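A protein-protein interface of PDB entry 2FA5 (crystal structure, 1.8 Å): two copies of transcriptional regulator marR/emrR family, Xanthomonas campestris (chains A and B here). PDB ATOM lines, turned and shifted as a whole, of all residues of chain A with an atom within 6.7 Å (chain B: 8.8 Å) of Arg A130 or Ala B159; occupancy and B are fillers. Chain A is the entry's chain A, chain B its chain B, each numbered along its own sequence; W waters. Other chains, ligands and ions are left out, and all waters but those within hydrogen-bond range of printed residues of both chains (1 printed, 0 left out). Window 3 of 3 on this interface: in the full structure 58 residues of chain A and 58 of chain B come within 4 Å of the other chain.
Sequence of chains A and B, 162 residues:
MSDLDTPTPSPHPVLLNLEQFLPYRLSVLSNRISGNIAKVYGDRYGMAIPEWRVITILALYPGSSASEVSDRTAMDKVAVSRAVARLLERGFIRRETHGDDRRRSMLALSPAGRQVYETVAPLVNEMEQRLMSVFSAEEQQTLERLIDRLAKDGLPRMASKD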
ATOM      1  N   ASN A  36      12.190  -9.725  -0.495  1.00  0.00           N
ATOM      2  CA  ASN A  36      11.871  -9.529   0.914  1.00  0.00           C
ATOM      3  C   ASN A  36      13.146  -9.589   1.748  1.00  0.00           C
ATOM      4  O   ASN A  36      13.310  -8.838   2.716  1.00  0.00           O
ATOM      5  CB  ASN A  36      10.864 -10.583   1.382  1.00  0.00           C
ATOM      6  CG  ASN A  36       9.450 -10.282   0.913  1.00  0.00           C
ATOM      7  OD1 ASN A  36       8.550 -11.112   1.033  1.00  0.00           O
ATOM      8  ND2 ASN A  36       9.249  -9.083   0.381  1.00  0.00           N
ATOM      9  N   LYS A  39      15.325  -6.380   1.696  1.00  0.00           N
ATOM     10  CA  LYS A  39      14.966  -5.223   2.504  1.00  0.00           C
ATOM     11  C   LYS A  39      15.900  -5.105   3.701  1.00  0.00           C
ATOM     12  O   LYS A  39      16.180  -4.003   4.179  1.00  0.00           O
ATOM     13  CB  LYS A  39      13.520  -5.335   2.984  1.00  0.00           C
ATOM     14  CG  LYS A  39      12.946  -4.021   3.483  1.00  0.00           C
ATOM     15  CD  LYS A  39      11.528  -4.182   3.994  1.00  0.00           C
ATOM     16  CE  LYS A  39      10.897  -2.827   4.259  1.00  0.00           C
ATOM     17  NZ  LYS A  39      11.728  -2.004   5.176  1.00  0.00           N
ATOM     18  N   VAL A  40      16.385  -6.245   4.184  1.00  0.00           N
ATOM     19  CA  VAL A  40      17.285  -6.260   5.329  1.00  0.00           C
ATOM     20  C   VAL A  40      18.548  -5.442   5.075  1.00  0.00           C
ATOM     21  O   VAL A  40      18.874  -4.539   5.847  1.00  0.00           O
ATOM     22  CB  VAL A  40      17.691  -7.703   5.705  1.00  0.00           C
ATOM     23  CG1 VAL A  40      18.720  -7.681   6.818  1.00  0.00           C
ATOM     24  CG2 VAL A  40      16.457  -8.490   6.141  1.00  0.00           C
ATOM     25  N   LEU A 123      19.888 -11.982  10.517  1.00  0.00           N
ATOM     26  CA  LEU A 123      18.552 -11.469  10.244  1.00  0.00           C
ATOM     27  C   LEU A 123      17.944 -12.170   9.036  1.00  0.00           C
ATOM     28  O   LEU A 123      16.740 -12.422   8.997  1.00  0.00           O
ATOM     29  CB  LEU A 123      18.609  -9.959  10.006  1.00  0.00           C
ATOM     30  CG  LEU A 123      19.069  -9.150  11.229  1.00  0.00           C
ATOM     31  CD1 LEU A 123      19.294  -7.695  10.836  1.00  0.00           C
ATOM     32  CD2 LEU A 123      18.029  -9.272  12.344  1.00  0.00           C
ATOM     33  N   ASN A 125      18.683 -15.184   8.164  1.00  0.00           N
ATOM     34  CA  ASN A 125      18.381 -16.529   8.652  1.00  0.00           C
ATOM     35  C   ASN A 125      17.023 -16.560   9.335  1.00  0.00           C
ATOM     36  O   ASN A 125      16.204 -17.434   9.060  1.00  0.00           O
ATOM     37  CB  ASN A 125      19.441 -17.001   9.648  1.00  0.00           C
ATOM     38  CG  ASN A 125      20.597 -17.702   8.981  1.00  0.00           C
ATOM     39  OD1 ASN A 125      20.403 -18.619   8.179  1.00  0.00           O
ATOM     40  ND2 ASN A 125      21.812 -17.289   9.317  1.00  0.00           N
ATOM     41  N   GLU A 126      16.795 -15.603  10.230  1.00  0.00           N
ATOM     42  CA  GLU A 126      15.537 -15.524  10.959  1.00  0.00           C
ATOM     43  C   GLU A 126      14.361 -15.282  10.022  1.00  0.00           C
ATOM     44  O   GLU A 126      13.273 -15.821  10.229  1.00  0.00           O
ATOM     45  CB  GLU A 126      15.599 -14.407  12.006  1.00  0.00           C
ATOM     46  CG  GLU A 126      16.731 -14.569  13.010  1.00  0.00           C
ATOM     47  CD  GLU A 126      16.708 -13.512  14.099  1.00  0.00           C
ATOM     48  OE1 GLU A 126      16.577 -12.314  13.769  1.00  0.00           O
ATOM     49  OE2 GLU A 126      16.828 -13.882  15.286  1.00  0.00           O
ATOM     50  N   MET A 127      14.574 -14.468   8.995  1.00  0.00           N
ATOM     51  CA  MET A 127      13.505 -14.187   8.049  1.00  0.00           C
ATOM     52  C   MET A 127      13.159 -15.435   7.247  1.00  0.00           C
ATOM     53  O   MET A 127      11.991 -15.696   6.967  1.00  0.00           O
ATOM     54  CB  MET A 127      13.905 -13.062   7.101  1.00  0.00           C
ATOM     55  CG  MET A 127      12.821 -12.713   6.108  1.00  0.00           C
ATOM     56  SD  MET A 127      13.300 -11.187   5.033  1.00  0.00           S
ATOM     57  CE  MET A 127      13.051  -9.794   6.360  1.00  0.00           C
ATOM     58  N   GLU A 128      14.177 -16.207   6.883  1.00  0.00           N
ATOM     59  CA  GLU A 128      13.962 -17.430   6.119  1.00  0.00           C
ATOM     60  C   GLU A 128      13.204 -18.447   6.969  1.00  0.00           C
ATOM     61  O   GLU A 128      12.396 -19.224   6.456  1.00  0.00           O
ATOM     62  CB  GLU A 128      15.305 -18.011   5.673  1.00  0.00           C
ATOM     63  CG  GLU A 128      15.207 -19.145   4.663  1.00  0.00           C
ATOM     64  CD  GLU A 128      14.971 -20.500   5.298  1.00  0.00           C
ATOM     65  OE1 GLU A 128      14.994 -20.601   6.545  1.00  0.00           O
ATOM     66  OE2 GLU A 128      14.772 -21.476   4.541  1.00  0.00           O
ATOM     67  N   GLN A 129      13.468 -18.440   8.271  1.00  0.00           N
ATOM     68  CA  GLN A 129      12.794 -19.362   9.179  1.00  0.00           C
ATOM     69  C   GLN A 129      11.309 -19.018   9.245  1.00  0.00           C
ATOM     70  O   GLN A 129      10.459 -19.909   9.317  1.00  0.00           O
ATOM     71  CB  GLN A 129      13.419 -19.287  10.575  1.00  0.00           C
ATOM     72  CG  GLN A 129      14.856 -19.779  10.634  1.00  0.00           C
ATOM     73  CD  GLN A 129      15.398 -19.831  12.054  1.00  0.00           C
ATOM     74  OE1 GLN A 129      14.874 -20.554  12.904  1.00  0.00           O
ATOM     75  NE2 GLN A 129      16.453 -19.064  12.316  1.00  0.00           N
ATOM     76  N   ARG A 130      11.000 -17.724   9.221  1.00  0.00           N
ATOM     77  CA  ARG A 130       9.609 -17.284   9.254  1.00  0.00           C
ATOM     78  C   ARG A 130       8.921 -17.722   7.966  1.00  0.00           C
ATOM     79  O   ARG A 130       7.752 -18.117   7.973  1.00  0.00           O
ATOM     80  CB  ARG A 130       9.522 -15.764   9.404  1.00  0.00           C
ATOM     81  CG  ARG A 130       9.962 -15.248  10.774  1.00  0.00           C
ATOM     82  CD  ARG A 130       9.485 -13.819  10.999  1.00  0.00           C
ATOM     83  NE  ARG A 130      10.196 -12.842  10.177  1.00  0.00           N
ATOM     84  CZ  ARG A 130      11.404 -12.364  10.463  1.00  0.00           C
ATOM     85  NH1 ARG A 130      12.043 -12.772  11.553  1.00  0.00           N
ATOM     86  NH2 ARG A 130      11.968 -11.466   9.667  1.00  0.00           N
ATOM     87  N   LEU A 131       9.652 -17.659   6.859  1.00  0.00           N
ATOM     88  CA  LEU A 131       9.112 -18.072   5.568  1.00  0.00           C
ATOM     89  C   LEU A 131       8.779 -19.562   5.568  1.00  0.00           C
ATOM     90  O   LEU A 131       7.703 -19.967   5.135  1.00  0.00           O
ATOM     91  CB  LEU A 131      10.126 -17.785   4.451  1.00  0.00           C
ATOM     92  CG  LEU A 131       9.916 -18.513   3.117  1.00  0.00           C
ATOM     93  CD1 LEU A 131       8.624 -18.043   2.458  1.00  0.00           C
ATOM     94  CD2 LEU A 131      11.108 -18.254   2.202  1.00  0.00           C
ATOM     95  N   MET A 132       9.708 -20.371   6.064  1.00  0.00           N
ATOM     96  CA  MET A 132       9.532 -21.819   6.085  1.00  0.00           C
ATOM     97  C   MET A 132       8.618 -22.339   7.183  1.00  0.00           C
ATOM     98  O   MET A 132       8.268 -23.523   7.188  1.00  0.00           O
ATOM     99  CB  MET A 132      10.893 -22.512   6.201  1.00  0.00           C
ATOM    100  CG  MET A 132      11.822 -22.226   5.042  1.00  0.00           C
ATOM    101  SD  MET A 132      10.979 -22.633   3.355  1.00  0.00           S
ATOM    102  CE  MET A 132      11.257 -24.543   3.355  1.00  0.00           C
ATOM    103  N   SER A 133       8.224 -21.462   8.102  1.00  0.00           N
ATOM    104  CA  SER A 133       7.359 -21.865   9.208  1.00  0.00           C
ATOM    105  C   SER A 133       5.994 -22.356   8.728  1.00  0.00           C
ATOM    106  O   SER A 133       5.239 -22.952   9.498  1.00  0.00           O
ATOM    107  CB  SER A 133       7.170 -20.703  10.192  1.00  0.00           C
ATOM    108  OG  SER A 133       6.338 -19.690   9.656  1.00  0.00           O
ATOM    109  N   VAL A 134       5.676 -22.107   7.460  1.00  0.00           N
ATOM    110  CA  VAL A 134       4.398 -22.542   6.907  1.00  0.00           C
ATOM    111  C   VAL A 134       4.409 -24.047   6.658  1.00  0.00           C
ATOM    112  O   VAL A 134       3.361 -24.661   6.474  1.00  0.00           O
ATOM    113  CB  VAL A 134       4.075 -21.827   5.576  1.00  0.00           C
ATOM    114  CG1 VAL A 134       3.868 -20.341   5.820  1.00  0.00           C
ATOM    115  CG2 VAL A 134       5.196 -22.056   4.572  1.00  0.00           C
ATOM    116  N   LEU B 150       4.068 -21.347  -0.302  1.00  0.00           N
ATOM    117  CA  LEU B 150       5.142 -20.419   0.038  1.00  0.00           C
ATOM    118  C   LEU B 150       4.792 -19.012  -0.420  1.00  0.00           C
ATOM    119  O   LEU B 150       5.034 -18.036   0.293  1.00  0.00           O
ATOM    120  CB  LEU B 150       6.459 -20.840  -0.619  1.00  0.00           C
ATOM    121  CG  LEU B 150       7.269 -21.915   0.101  1.00  0.00           C
ATOM    122  CD1 LEU B 150       8.547 -22.205  -0.683  1.00  0.00           C
ATOM    123  CD2 LEU B 150       7.606 -21.434   1.508  1.00  0.00           C
ATOM    124  N   ASP B 153       1.134 -17.998   1.757  1.00  0.00           N
ATOM    125  CA  ASP B 153       1.223 -17.894   3.210  1.00  0.00           C
ATOM    126  C   ASP B 153       2.621 -17.695   3.774  1.00  0.00           C
ATOM    127  O   ASP B 153       2.774 -17.258   4.912  1.00  0.00           O
ATOM    128  CB  ASP B 153       0.582 -19.125   3.857  1.00  0.00           C
ATOM    129  CG  ASP B 153      -0.907 -19.219   3.577  1.00  0.00           C
ATOM    130  OD1 ASP B 153      -1.284 -19.359   2.395  1.00  0.00           O
ATOM    131  OD2 ASP B 153      -1.701 -19.144   4.540  1.00  0.00           O
ATOM    132  N   GLY B 154       3.639 -18.021   2.988  1.00  0.00           N
ATOM    133  CA  GLY B 154       5.000 -17.856   3.469  1.00  0.00           C
ATOM    134  C   GLY B 154       5.538 -16.444   3.310  1.00  0.00           C
ATOM    135  O   GLY B 154       6.118 -15.885   4.242  1.00  0.00           O
ATOM    136  N   LEU B 155       5.350 -15.864   2.130  1.00  0.00           N
ATOM    137  CA  LEU B 155       5.841 -14.517   1.861  1.00  0.00           C
ATOM    138  C   LEU B 155       5.422 -13.453   2.875  1.00  0.00           C
ATOM    139  O   LEU B 155       6.252 -12.668   3.327  1.00  0.00           O
ATOM    140  CB  LEU B 155       5.428 -14.073   0.456  1.00  0.00           C
ATOM    141  CG  LEU B 155       6.195 -14.729  -0.696  1.00  0.00           C
ATOM    142  CD1 LEU B 155       5.625 -14.255  -2.015  1.00  0.00           C
ATOM    143  CD2 LEU B 155       7.671 -14.384  -0.607  1.00  0.00           C
ATOM    144  N   PRO B 156       4.131 -13.407   3.244  1.00  0.00           N
ATOM    145  CA  PRO B 156       3.701 -12.392   4.212  1.00  0.00           C
ATOM    146  C   PRO B 156       4.307 -12.516   5.609  1.00  0.00           C
ATOM    147  O   PRO B 156       4.260 -11.568   6.395  1.00  0.00           O
ATOM    148  CB  PRO B 156       2.177 -12.548   4.219  1.00  0.00           C
ATOM    149  CG  PRO B 156       1.989 -13.999   3.920  1.00  0.00           C
ATOM    150  CD  PRO B 156       2.989 -14.232   2.807  1.00  0.00           C
ATOM    151  N   ARG B 157       4.875 -13.677   5.924  1.00  0.00           N
ATOM    152  CA  ARG B 157       5.473 -13.888   7.240  1.00  0.00           C
ATOM    153  C   ARG B 157       6.916 -13.407   7.326  1.00  0.00           C
ATOM    154  O   ARG B 157       7.488 -13.335   8.413  1.00  0.00           O
ATOM    155  CB  ARG B 157       5.429 -15.370   7.617  1.00  0.00           C
ATOM    156  CG  ARG B 157       4.033 -15.933   7.810  1.00  0.00           C
ATOM    157  CD  ARG B 157       4.086 -17.326   8.421  1.00  0.00           C
ATOM    158  NE  ARG B 157       2.753 -17.894   8.605  1.00  0.00           N
ATOM    159  CZ  ARG B 157       2.505 -19.051   9.214  1.00  0.00           C
ATOM    160  NH1 ARG B 157       3.501 -19.776   9.706  1.00  0.00           N
ATOM    161  NH2 ARG B 157       1.256 -19.483   9.333  1.00  0.00           N
ATOM    162  N   MET B 158       7.501 -13.067   6.182  1.00  0.00           N
ATOM    163  CA  MET B 158       8.890 -12.632   6.141  1.00  0.00           C
ATOM    164  C   MET B 158       9.203 -11.264   6.744  1.00  0.00           C
ATOM    165  O   MET B 158      10.136 -11.140   7.539  1.00  0.00           O
ATOM    166  CB  MET B 158       9.397 -12.690   4.702  1.00  0.00           C
ATOM    167  CG  MET B 158       9.411 -14.103   4.140  1.00  0.00           C
ATOM    168  SD  MET B 158      10.132 -14.204   2.343  1.00  0.00           S
ATOM    169  CE  MET B 158      12.001 -13.948   2.769  1.00  0.00           C
ATOM    170  N   ALA B 159       8.439 -10.241   6.370  1.00  0.00           N
ATOM    171  CA  ALA B 159       8.680  -8.896   6.891  1.00  0.00           C
ATOM    172  C   ALA B 159       8.829  -8.900   8.408  1.00  0.00           C
ATOM    173  O   ALA B 159       8.134  -9.702   9.066  1.00  0.00           O
ATOM    174  CB  ALA B 159       7.543  -7.963   6.482  1.00  0.00           C
HETATM  175  O   HOH W   1       2.650 -22.028  11.356  1.00  0.00           O
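The side-chain amide oxygen of Asn A36 sits close to the side-chain sulfur of Met B158, 3.7 Å away. O of Arg B157 lies within hydrogen-bond range of NE of Arg A130 (3.3 Å). NH2 of Arg A130 sits at hydrogen-bond distance from O of Met B158. NH1 of Arg B157 is in hydrogen-bond range of OG of Ser A133.
The backbone carbonyl oxygen of Arg A130 sits at hydrogen-bond distance from the side-chain hydroxyl of Ser A133. The backbone NH (N) of Leu B155 lies within hydrogen-bond range of the backbone carbonyl oxygen (O) of Leu B150.
Among the printed residues, pairs that only touch across the chains: Val A134 with Asp B153 (3.4 Å), Met A127 with Met B158 (3.4 Å), Leu A131 with Gly B154 (3.6 Å), Asn A36 with Leu B155 (3.6 Å), Val A134 with Gly B154 (3.6 Å), Leu A131 with Leu B150 (3.7 Å), Leu A131 with Met B158 (3.8 Å), Val A134 with Arg B157 (3.9 Å), Arg A130 with Ala B159 (3.9 Å), Leu A131 with Leu B155 (3.9 Å) and Val A134 with Leu B150 (3.9 Å).
Leu A123 touches none of the printed residues of chain B. Of the printed residues of chain B, Met A127 touches Met B158 (3.4 Å). Glu A128 touches none of the printed residues of chain B. Arg A130 touches just these residues of chain B: Arg B157, Met B158 and Ala B159. Of the printed residues of chain B, Leu A131 touches Leu B150, Gly B154, Leu B155 and Met B158. Of the printed residues of chain B, Val A134 touches Leu B150, Asp B153, Gly B154 and Arg B157. Printed residues of chain A within 4 Å of Leu B150: Leu A131 (3.7 Å) and Val A134 (3.9 Å). Printed residues of chain A within 4 Å of Gly B154: Leu A131 and Val A134. Of chain A, only Arg A130 (3.9 Å) comes within 4 Å of Ala B159. The nearest residue of chain B that does not touch Arg A130 is Gly B154 (4.6 Å).
Of the 8 printed residues of chain B, 7 touch a printed residue of chain A. Printed residues of chain B that touch a printed residue of chain A: Leu B150, Asp B153, Gly B154, Leu B155, Arg B157, Met B158 and Ala B159. Hydrophobic or aromatic side chains of chain B that line the printed part of chain A: Leu B150, Leu B155 and Met B158. Of the 14 printed residues of chain A, 6 touch a printed residue of chain B. Printed residues of chain A that touch a printed residue of chain B: Asn A36, Met A127, Arg A130, Leu A131, Ser A133 and Val A134. Hydrophobic or aromatic side chains of chain A within 4 Å of the printed part of chain B: Met A127, Leu A131 and Val A134. Among the printed residues, 15 pairs touch across the chains.
No position is printed for both chains.
Water W1 bridges the guanidinium group of Arg B157 (2.9 Å) and the backbone carbonyl oxygen of Ser A133 (3.3 Å).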
